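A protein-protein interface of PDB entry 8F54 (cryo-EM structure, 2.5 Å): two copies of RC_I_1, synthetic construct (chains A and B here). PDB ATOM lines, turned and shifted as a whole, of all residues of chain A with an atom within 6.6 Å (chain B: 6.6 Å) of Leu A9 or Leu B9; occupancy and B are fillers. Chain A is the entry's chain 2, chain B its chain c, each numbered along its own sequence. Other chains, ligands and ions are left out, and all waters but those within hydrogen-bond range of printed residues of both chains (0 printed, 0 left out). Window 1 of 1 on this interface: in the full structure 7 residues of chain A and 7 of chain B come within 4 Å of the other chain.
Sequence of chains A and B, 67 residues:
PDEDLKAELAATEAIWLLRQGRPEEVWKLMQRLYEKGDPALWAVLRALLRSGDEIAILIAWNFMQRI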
ATOM      1  N   ASP A   4     -26.889 -32.196 -36.528  1.00  0.00           N
ATOM      2  CA  ASP A   4     -27.347 -32.266 -35.145  1.00  0.00           C
ATOM      3  C   ASP A   4     -26.182 -32.179 -34.167  1.00  0.00           C
ATOM      4  O   ASP A   4     -26.312 -31.559 -33.106  1.00  0.00           O
ATOM      5  CB  ASP A   4     -28.136 -33.555 -34.924  1.00  0.00           C
ATOM      6  CG  ASP A   4     -28.814 -33.600 -33.570  1.00  0.00           C
ATOM      7  OD1 ASP A   4     -29.594 -32.675 -33.262  1.00  0.00           O
ATOM      8  OD2 ASP A   4     -28.577 -34.566 -32.816  1.00  0.00           O
ATOM      9  N   LEU A   5     -25.035 -32.769 -34.510  1.00  0.00           N
ATOM     10  CA  LEU A   5     -23.858 -32.627 -33.659  1.00  0.00           C
ATOM     11  C   LEU A   5     -23.425 -31.170 -33.578  1.00  0.00           C
ATOM     12  O   LEU A   5     -23.107 -30.664 -32.495  1.00  0.00           O
ATOM     13  CB  LEU A   5     -22.715 -33.499 -34.182  1.00  0.00           C
ATOM     14  CG  LEU A   5     -21.377 -33.337 -33.451  1.00  0.00           C
ATOM     15  CD1 LEU A   5     -21.501 -33.724 -31.984  1.00  0.00           C
ATOM     16  CD2 LEU A   5     -20.284 -34.145 -34.123  1.00  0.00           C
ATOM     17  N   LYS A   6     -23.384 -30.484 -34.720  1.00  0.00           N
ATOM     18  CA  LYS A   6     -22.996 -29.078 -34.719  1.00  0.00           C
ATOM     19  C   LYS A   6     -23.978 -28.236 -33.914  1.00  0.00           C
ATOM     20  O   LYS A   6     -23.573 -27.316 -33.198  1.00  0.00           O
ATOM     21  CB  LYS A   6     -22.880 -28.568 -36.152  1.00  0.00           C
ATOM     22  CG  LYS A   6     -21.624 -29.047 -36.850  1.00  0.00           C
ATOM     23  CD  LYS A   6     -21.525 -28.523 -38.267  1.00  0.00           C
ATOM     24  CE  LYS A   6     -20.219 -28.948 -38.917  1.00  0.00           C
ATOM     25  NZ  LYS A   6     -20.126 -28.521 -40.336  1.00  0.00           N
ATOM     26  N   ALA A   7     -25.273 -28.536 -34.014  1.00  0.00           N
ATOM     27  CA  ALA A   7     -26.257 -27.827 -33.203  1.00  0.00           C
ATOM     28  C   ALA A   7     -26.008 -28.055 -31.716  1.00  0.00           C
ATOM     29  O   ALA A   7     -26.045 -27.113 -30.913  1.00  0.00           O
ATOM     30  CB  ALA A   7     -27.666 -28.270 -33.595  1.00  0.00           C
ATOM     31  N   GLU A   8     -25.745 -29.308 -31.332  1.00  0.00           N
ATOM     32  CA  GLU A   8     -25.478 -29.619 -29.930  1.00  0.00           C
ATOM     33  C   GLU A   8     -24.245 -28.885 -29.427  1.00  0.00           C
ATOM     34  O   GLU A   8     -24.241 -28.342 -28.316  1.00  0.00           O
ATOM     35  CB  GLU A   8     -25.291 -31.126 -29.756  1.00  0.00           C
ATOM     36  CG  GLU A   8     -26.567 -31.936 -29.763  1.00  0.00           C
ATOM     37  CD  GLU A   8     -27.338 -31.805 -28.468  1.00  0.00           C
ATOM     38  OE1 GLU A   8     -27.793 -30.686 -28.155  1.00  0.00           O
ATOM     39  OE2 GLU A   8     -27.474 -32.819 -27.754  1.00  0.00           O
ATOM     40  N   LEU A   9     -23.186 -28.855 -30.234  1.00  0.00           N
ATOM     41  CA  LEU A   9     -21.958 -28.192 -29.817  1.00  0.00           C
ATOM     42  C   LEU A   9     -22.151 -26.686 -29.717  1.00  0.00           C
ATOM     43  O   LEU A   9     -21.631 -26.049 -28.795  1.00  0.00           O
ATOM     44  CB  LEU A   9     -20.826 -28.530 -30.785  1.00  0.00           C
ATOM     45  CG  LEU A   9     -20.402 -30.000 -30.818  1.00  0.00           C
ATOM     46  CD1 LEU A   9     -19.364 -30.231 -31.897  1.00  0.00           C
ATOM     47  CD2 LEU A   9     -19.876 -30.457 -29.464  1.00  0.00           C
ATOM     48  N   ALA A  10     -22.889 -26.095 -30.660  1.00  0.00           N
ATOM     49  CA  ALA A  10     -23.167 -24.666 -30.588  1.00  0.00           C
ATOM     50  C   ALA A  10     -23.954 -24.323 -29.331  1.00  0.00           C
ATOM     51  O   ALA A  10     -23.639 -23.347 -28.640  1.00  0.00           O
ATOM     52  CB  ALA A  10     -23.921 -24.216 -31.838  1.00  0.00           C
ATOM     53  N   ALA A  11     -24.978 -25.116 -29.009  1.00  0.00           N
ATOM     54  CA  ALA A  11     -25.750 -24.848 -27.800  1.00  0.00           C
ATOM     55  C   ALA A  11     -24.905 -25.033 -26.546  1.00  0.00           C
ATOM     56  O   ALA A  11     -25.033 -24.258 -25.588  1.00  0.00           O
ATOM     57  CB  ALA A  11     -26.981 -25.752 -27.755  1.00  0.00           C
ATOM     58  N   THR A  12     -24.020 -26.033 -26.542  1.00  0.00           N
ATOM     59  CA  THR A  12     -23.148 -26.241 -25.393  1.00  0.00           C
ATOM     60  C   THR A  12     -22.209 -25.056 -25.202  1.00  0.00           C
ATOM     61  O   THR A  12     -22.041 -24.561 -24.083  1.00  0.00           O
ATOM     62  CB  THR A  12     -22.355 -27.538 -25.570  1.00  0.00           C
ATOM     63  OG1 THR A  12     -23.261 -28.646 -25.625  1.00  0.00           O
ATOM     64  CG2 THR A  12     -21.378 -27.748 -24.420  1.00  0.00           C
ATOM     65  N   GLU A  13     -21.591 -24.587 -26.286  1.00  0.00           N
ATOM     66  CA  GLU A  13     -20.703 -23.434 -26.186  1.00  0.00           C
ATOM     67  C   GLU A  13     -21.457 -22.192 -25.734  1.00  0.00           C
ATOM     68  O   GLU A  13     -20.947 -21.408 -24.928  1.00  0.00           O
ATOM     69  CB  GLU A  13     -20.010 -23.179 -27.523  1.00  0.00           C
ATOM     70  CG  GLU A  13     -19.165 -21.916 -27.543  1.00  0.00           C
ATOM     71  CD  GLU A  13     -18.303 -21.816 -28.783  1.00  0.00           C
ATOM     72  OE1 GLU A  13     -18.239 -22.805 -29.542  1.00  0.00           O
ATOM     73  OE2 GLU A  13     -17.688 -20.751 -29.003  1.00  0.00           O
ATOM     74  N   ALA A  14     -22.667 -21.979 -26.259  1.00  0.00           N
ATOM     75  CA  ALA A  14     -23.446 -20.811 -25.864  1.00  0.00           C
ATOM     76  C   ALA A  14     -23.757 -20.839 -24.374  1.00  0.00           C
ATOM     77  O   ALA A  14     -23.572 -19.839 -23.670  1.00  0.00           O
ATOM     78  CB  ALA A  14     -24.735 -20.743 -26.681  1.00  0.00           C
ATOM     79  N   LEU A  29     -21.495 -15.050 -31.193  1.00  0.00           N
ATOM     80  CA  LEU A  29     -21.724 -16.396 -31.703  1.00  0.00           C
ATOM     81  C   LEU A  29     -23.006 -16.452 -32.521  1.00  0.00           C
ATOM     82  O   LEU A  29     -23.028 -16.992 -33.637  1.00  0.00           O
ATOM     83  CB  LEU A  29     -21.771 -17.378 -30.529  1.00  0.00           C
ATOM     84  CG  LEU A  29     -22.234 -18.813 -30.781  1.00  0.00           C
ATOM     85  CD1 LEU A  29     -21.301 -19.530 -31.736  1.00  0.00           C
ATOM     86  CD2 LEU A  29     -22.332 -19.560 -29.466  1.00  0.00           C
ATOM     87  N   ASP B   4     -11.700 -25.705 -20.139  1.00  0.00           N
ATOM     88  CA  ASP B   4     -12.988 -26.206 -19.677  1.00  0.00           C
ATOM     89  C   ASP B   4     -14.004 -26.260 -20.811  1.00  0.00           C
ATOM     90  O   ASP B   4     -14.803 -27.201 -20.880  1.00  0.00           O
ATOM     91  CB  ASP B   4     -13.506 -25.331 -18.537  1.00  0.00           C
ATOM     92  CG  ASP B   4     -14.745 -25.902 -17.878  1.00  0.00           C
ATOM     93  OD1 ASP B   4     -14.681 -27.041 -17.372  1.00  0.00           O
ATOM     94  OD2 ASP B   4     -15.782 -25.206 -17.858  1.00  0.00           O
ATOM     95  N   LEU B   5     -13.982 -25.278 -21.715  1.00  0.00           N
ATOM     96  CA  LEU B   5     -14.872 -25.326 -22.869  1.00  0.00           C
ATOM     97  C   LEU B   5     -14.556 -26.530 -23.746  1.00  0.00           C
ATOM     98  O   LEU B   5     -15.463 -27.229 -24.209  1.00  0.00           O
ATOM     99  CB  LEU B   5     -14.763 -24.031 -23.677  1.00  0.00           C
ATOM    100  CG  LEU B   5     -15.542 -24.010 -24.999  1.00  0.00           C
ATOM    101  CD1 LEU B   5     -17.033 -24.193 -24.759  1.00  0.00           C
ATOM    102  CD2 LEU B   5     -15.278 -22.730 -25.767  1.00  0.00           C
ATOM    103  N   LYS B   6     -13.271 -26.773 -24.003  1.00  0.00           N
ATOM    104  CA  LYS B   6     -12.894 -27.919 -24.823  1.00  0.00           C
ATOM    105  C   LYS B   6     -13.299 -29.230 -24.159  1.00  0.00           C
ATOM    106  O   LYS B   6     -13.746 -30.162 -24.836  1.00  0.00           O
ATOM    107  CB  LYS B   6     -11.395 -27.886 -25.107  1.00  0.00           C
ATOM    108  CG  LYS B   6     -11.011 -26.809 -26.099  1.00  0.00           C
ATOM    109  CD  LYS B   6      -9.523 -26.792 -26.373  1.00  0.00           C
ATOM    110  CE  LYS B   6      -9.176 -25.753 -27.424  1.00  0.00           C
ATOM    111  NZ  LYS B   6      -7.718 -25.691 -27.702  1.00  0.00           N
ATOM    112  N   ALA B   7     -13.157 -29.319 -22.837  1.00  0.00           N
ATOM    113  CA  ALA B   7     -13.612 -30.512 -22.129  1.00  0.00           C
ATOM    114  C   ALA B   7     -15.119 -30.696 -22.278  1.00  0.00           C
ATOM    115  O   ALA B   7     -15.602 -31.808 -22.530  1.00  0.00           O
ATOM    116  CB  ALA B   7     -13.216 -30.421 -20.657  1.00  0.00           C
ATOM    117  N   GLU B   8     -15.878 -29.606 -22.134  1.00  0.00           N
ATOM    118  CA  GLU B   8     -17.329 -29.679 -22.283  1.00  0.00           C
ATOM    119  C   GLU B   8     -17.715 -30.139 -23.682  1.00  0.00           C
ATOM    120  O   GLU B   8     -18.604 -30.982 -23.847  1.00  0.00           O
ATOM    121  CB  GLU B   8     -17.949 -28.312 -21.996  1.00  0.00           C
ATOM    122  CG  GLU B   8     -18.066 -27.957 -20.532  1.00  0.00           C
ATOM    123  CD  GLU B   8     -19.301 -28.553 -19.893  1.00  0.00           C
ATOM    124  OE1 GLU B   8     -19.773 -29.598 -20.381  1.00  0.00           O
ATOM    125  OE2 GLU B   8     -19.810 -27.967 -18.913  1.00  0.00           O
ATOM    126  N   LEU B   9     -17.052 -29.596 -24.701  1.00  0.00           N
ATOM    127  CA  LEU B   9     -17.374 -29.965 -26.073  1.00  0.00           C
ATOM    128  C   LEU B   9     -17.006 -31.414 -26.355  1.00  0.00           C
ATOM    129  O   LEU B   9     -17.751 -32.126 -27.039  1.00  0.00           O
ATOM    130  CB  LEU B   9     -16.664 -29.026 -27.048  1.00  0.00           C
ATOM    131  CG  LEU B   9     -17.116 -27.563 -26.999  1.00  0.00           C
ATOM    132  CD1 LEU B   9     -16.234 -26.707 -27.886  1.00  0.00           C
ATOM    133  CD2 LEU B   9     -18.577 -27.421 -27.400  1.00  0.00           C
ATOM    134  N   ALA B  10     -15.859 -31.869 -25.846  1.00  0.00           N
ATOM    135  CA  ALA B  10     -15.469 -33.262 -26.034  1.00  0.00           C
ATOM    136  C   ALA B  10     -16.479 -34.203 -25.391  1.00  0.00           C
ATOM    137  O   ALA B  10     -16.879 -35.205 -25.994  1.00  0.00           O
ATOM    138  CB  ALA B  10     -14.072 -33.492 -25.459  1.00  0.00           C
ATOM    139  N   ALA B  11     -16.913 -33.893 -24.168  1.00  0.00           N
ATOM    140  CA  ALA B  11     -17.901 -34.744 -23.511  1.00  0.00           C
ATOM    141  C   ALA B  11     -19.234 -34.721 -24.246  1.00  0.00           C
ATOM    142  O   ALA B  11     -19.902 -35.758 -24.358  1.00  0.00           O
ATOM    143  CB  ALA B  11     -18.081 -34.310 -22.058  1.00  0.00           C
ATOM    144  N   THR B  12     -19.628 -33.560 -24.773  1.00  0.00           N
ATOM    145  CA  THR B  12     -20.877 -33.477 -25.522  1.00  0.00           C
ATOM    146  C   THR B  12     -20.807 -34.323 -26.786  1.00  0.00           C
ATOM    147  O   THR B  12     -21.739 -35.073 -27.094  1.00  0.00           O
ATOM    148  CB  THR B  12     -21.186 -32.016 -25.860  1.00  0.00           C
ATOM    149  OG1 THR B  12     -21.358 -31.273 -24.649  1.00  0.00           O
ATOM    150  CG2 THR B  12     -22.450 -31.902 -26.700  1.00  0.00           C
ATOM    151  N   GLU B  13     -19.704 -34.221 -27.529  1.00  0.00           N
ATOM    152  CA  GLU B  13     -19.550 -35.029 -28.733  1.00  0.00           C
ATOM    153  C   GLU B  13     -19.529 -36.515 -28.401  1.00  0.00           C
ATOM    154  O   GLU B  13     -20.116 -37.325 -29.124  1.00  0.00           O
ATOM    155  CB  GLU B  13     -18.279 -34.634 -29.481  1.00  0.00           C
ATOM    156  CG  GLU B  13     -17.983 -35.510 -30.687  1.00  0.00           C
ATOM    157  CD  GLU B  13     -16.866 -34.956 -31.543  1.00  0.00           C
ATOM    158  OE1 GLU B  13     -16.364 -33.858 -31.225  1.00  0.00           O
ATOM    159  OE2 GLU B  13     -16.487 -35.613 -32.536  1.00  0.00           O
ATOM    160  N   ALA B  14     -18.842 -36.897 -27.322  1.00  0.00           N
ATOM    161  CA  ALA B  14     -18.788 -38.304 -26.942  1.00  0.00           C
ATOM    162  C   ALA B  14     -20.178 -38.841 -26.632  1.00  0.00           C
ATOM    163  O   ALA B  14     -20.568 -39.912 -27.116  1.00  0.00           O
ATOM    164  CB  ALA B  14     -17.863 -38.485 -25.739  1.00  0.00           C
ATOM    165  N   LEU B  29     -12.211 -41.230 -30.675  1.00  0.00           N
ATOM    166  CA  LEU B  29     -12.102 -39.928 -30.031  1.00  0.00           C
ATOM    167  C   LEU B  29     -11.208 -40.006 -28.801  1.00  0.00           C
ATOM    168  O   LEU B  29     -10.313 -39.173 -28.609  1.00  0.00           O
ATOM    169  CB  LEU B  29     -13.503 -39.429 -29.668  1.00  0.00           C
ATOM    170  CG  LEU B  29     -13.645 -38.197 -28.774  1.00  0.00           C
ATOM    171  CD1 LEU B  29     -13.063 -36.970 -29.443  1.00  0.00           C
ATOM    172  CD2 LEU B  29     -15.106 -37.978 -28.429  1.00  0.00           C
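Leu A9 touches its own counterpart, Leu B9. Thr B12 touches its own counterpart, Thr A12. 12 positions are printed for both chains. Of the 2 pairs that touch across the chains among the printed residues, 2 have their exchanged pair printed and touching as well.
Among the printed residues, merely in contact across the chains: Leu A9 with Leu B9 (3.6 Å).
Leu A9 touches just one residue of chain B: Leu B9. Leu B9 touches one residue of chain A. Of the printed residues of chain A, Thr B12 touches Thr A12 (3.4 Å). Printed residues of chain B within 4 Å of Thr A12: Thr B12 (3.4 Å). Ala B11 touches none of the printed residues of chain A.
OG1 of Thr A12 is in hydrogen-bond range of OG1 of Thr B12, at 3.4 Å.
Printed residues of chain A that touch a printed residue of chain B: Leu A9 and Thr A12. Hydrophobic or aromatic side chains of chain A that line the printed part of chain B: Leu A9. Printed residues of chain B that touch a printed residue of chain A: Leu B9 and Thr B12. Hydrophobic or aromatic side chains of chain B that line the printed part of chain A: Leu B9. Among the printed residues, no Asp or Glu carboxylate lies within 4 Å of a Lys or Arg side-chain nitrogen of the other chain.
The side-chain hydroxyl (OG1) of Thr B12 lies within hydrogen-bond range of the backbone carbonyl oxygen (O) of Glu B8 (2.9 Å). OG1 of Thr A12 sits at hydrogen-bond distance from O of Glu A8, 2.9 Å away.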
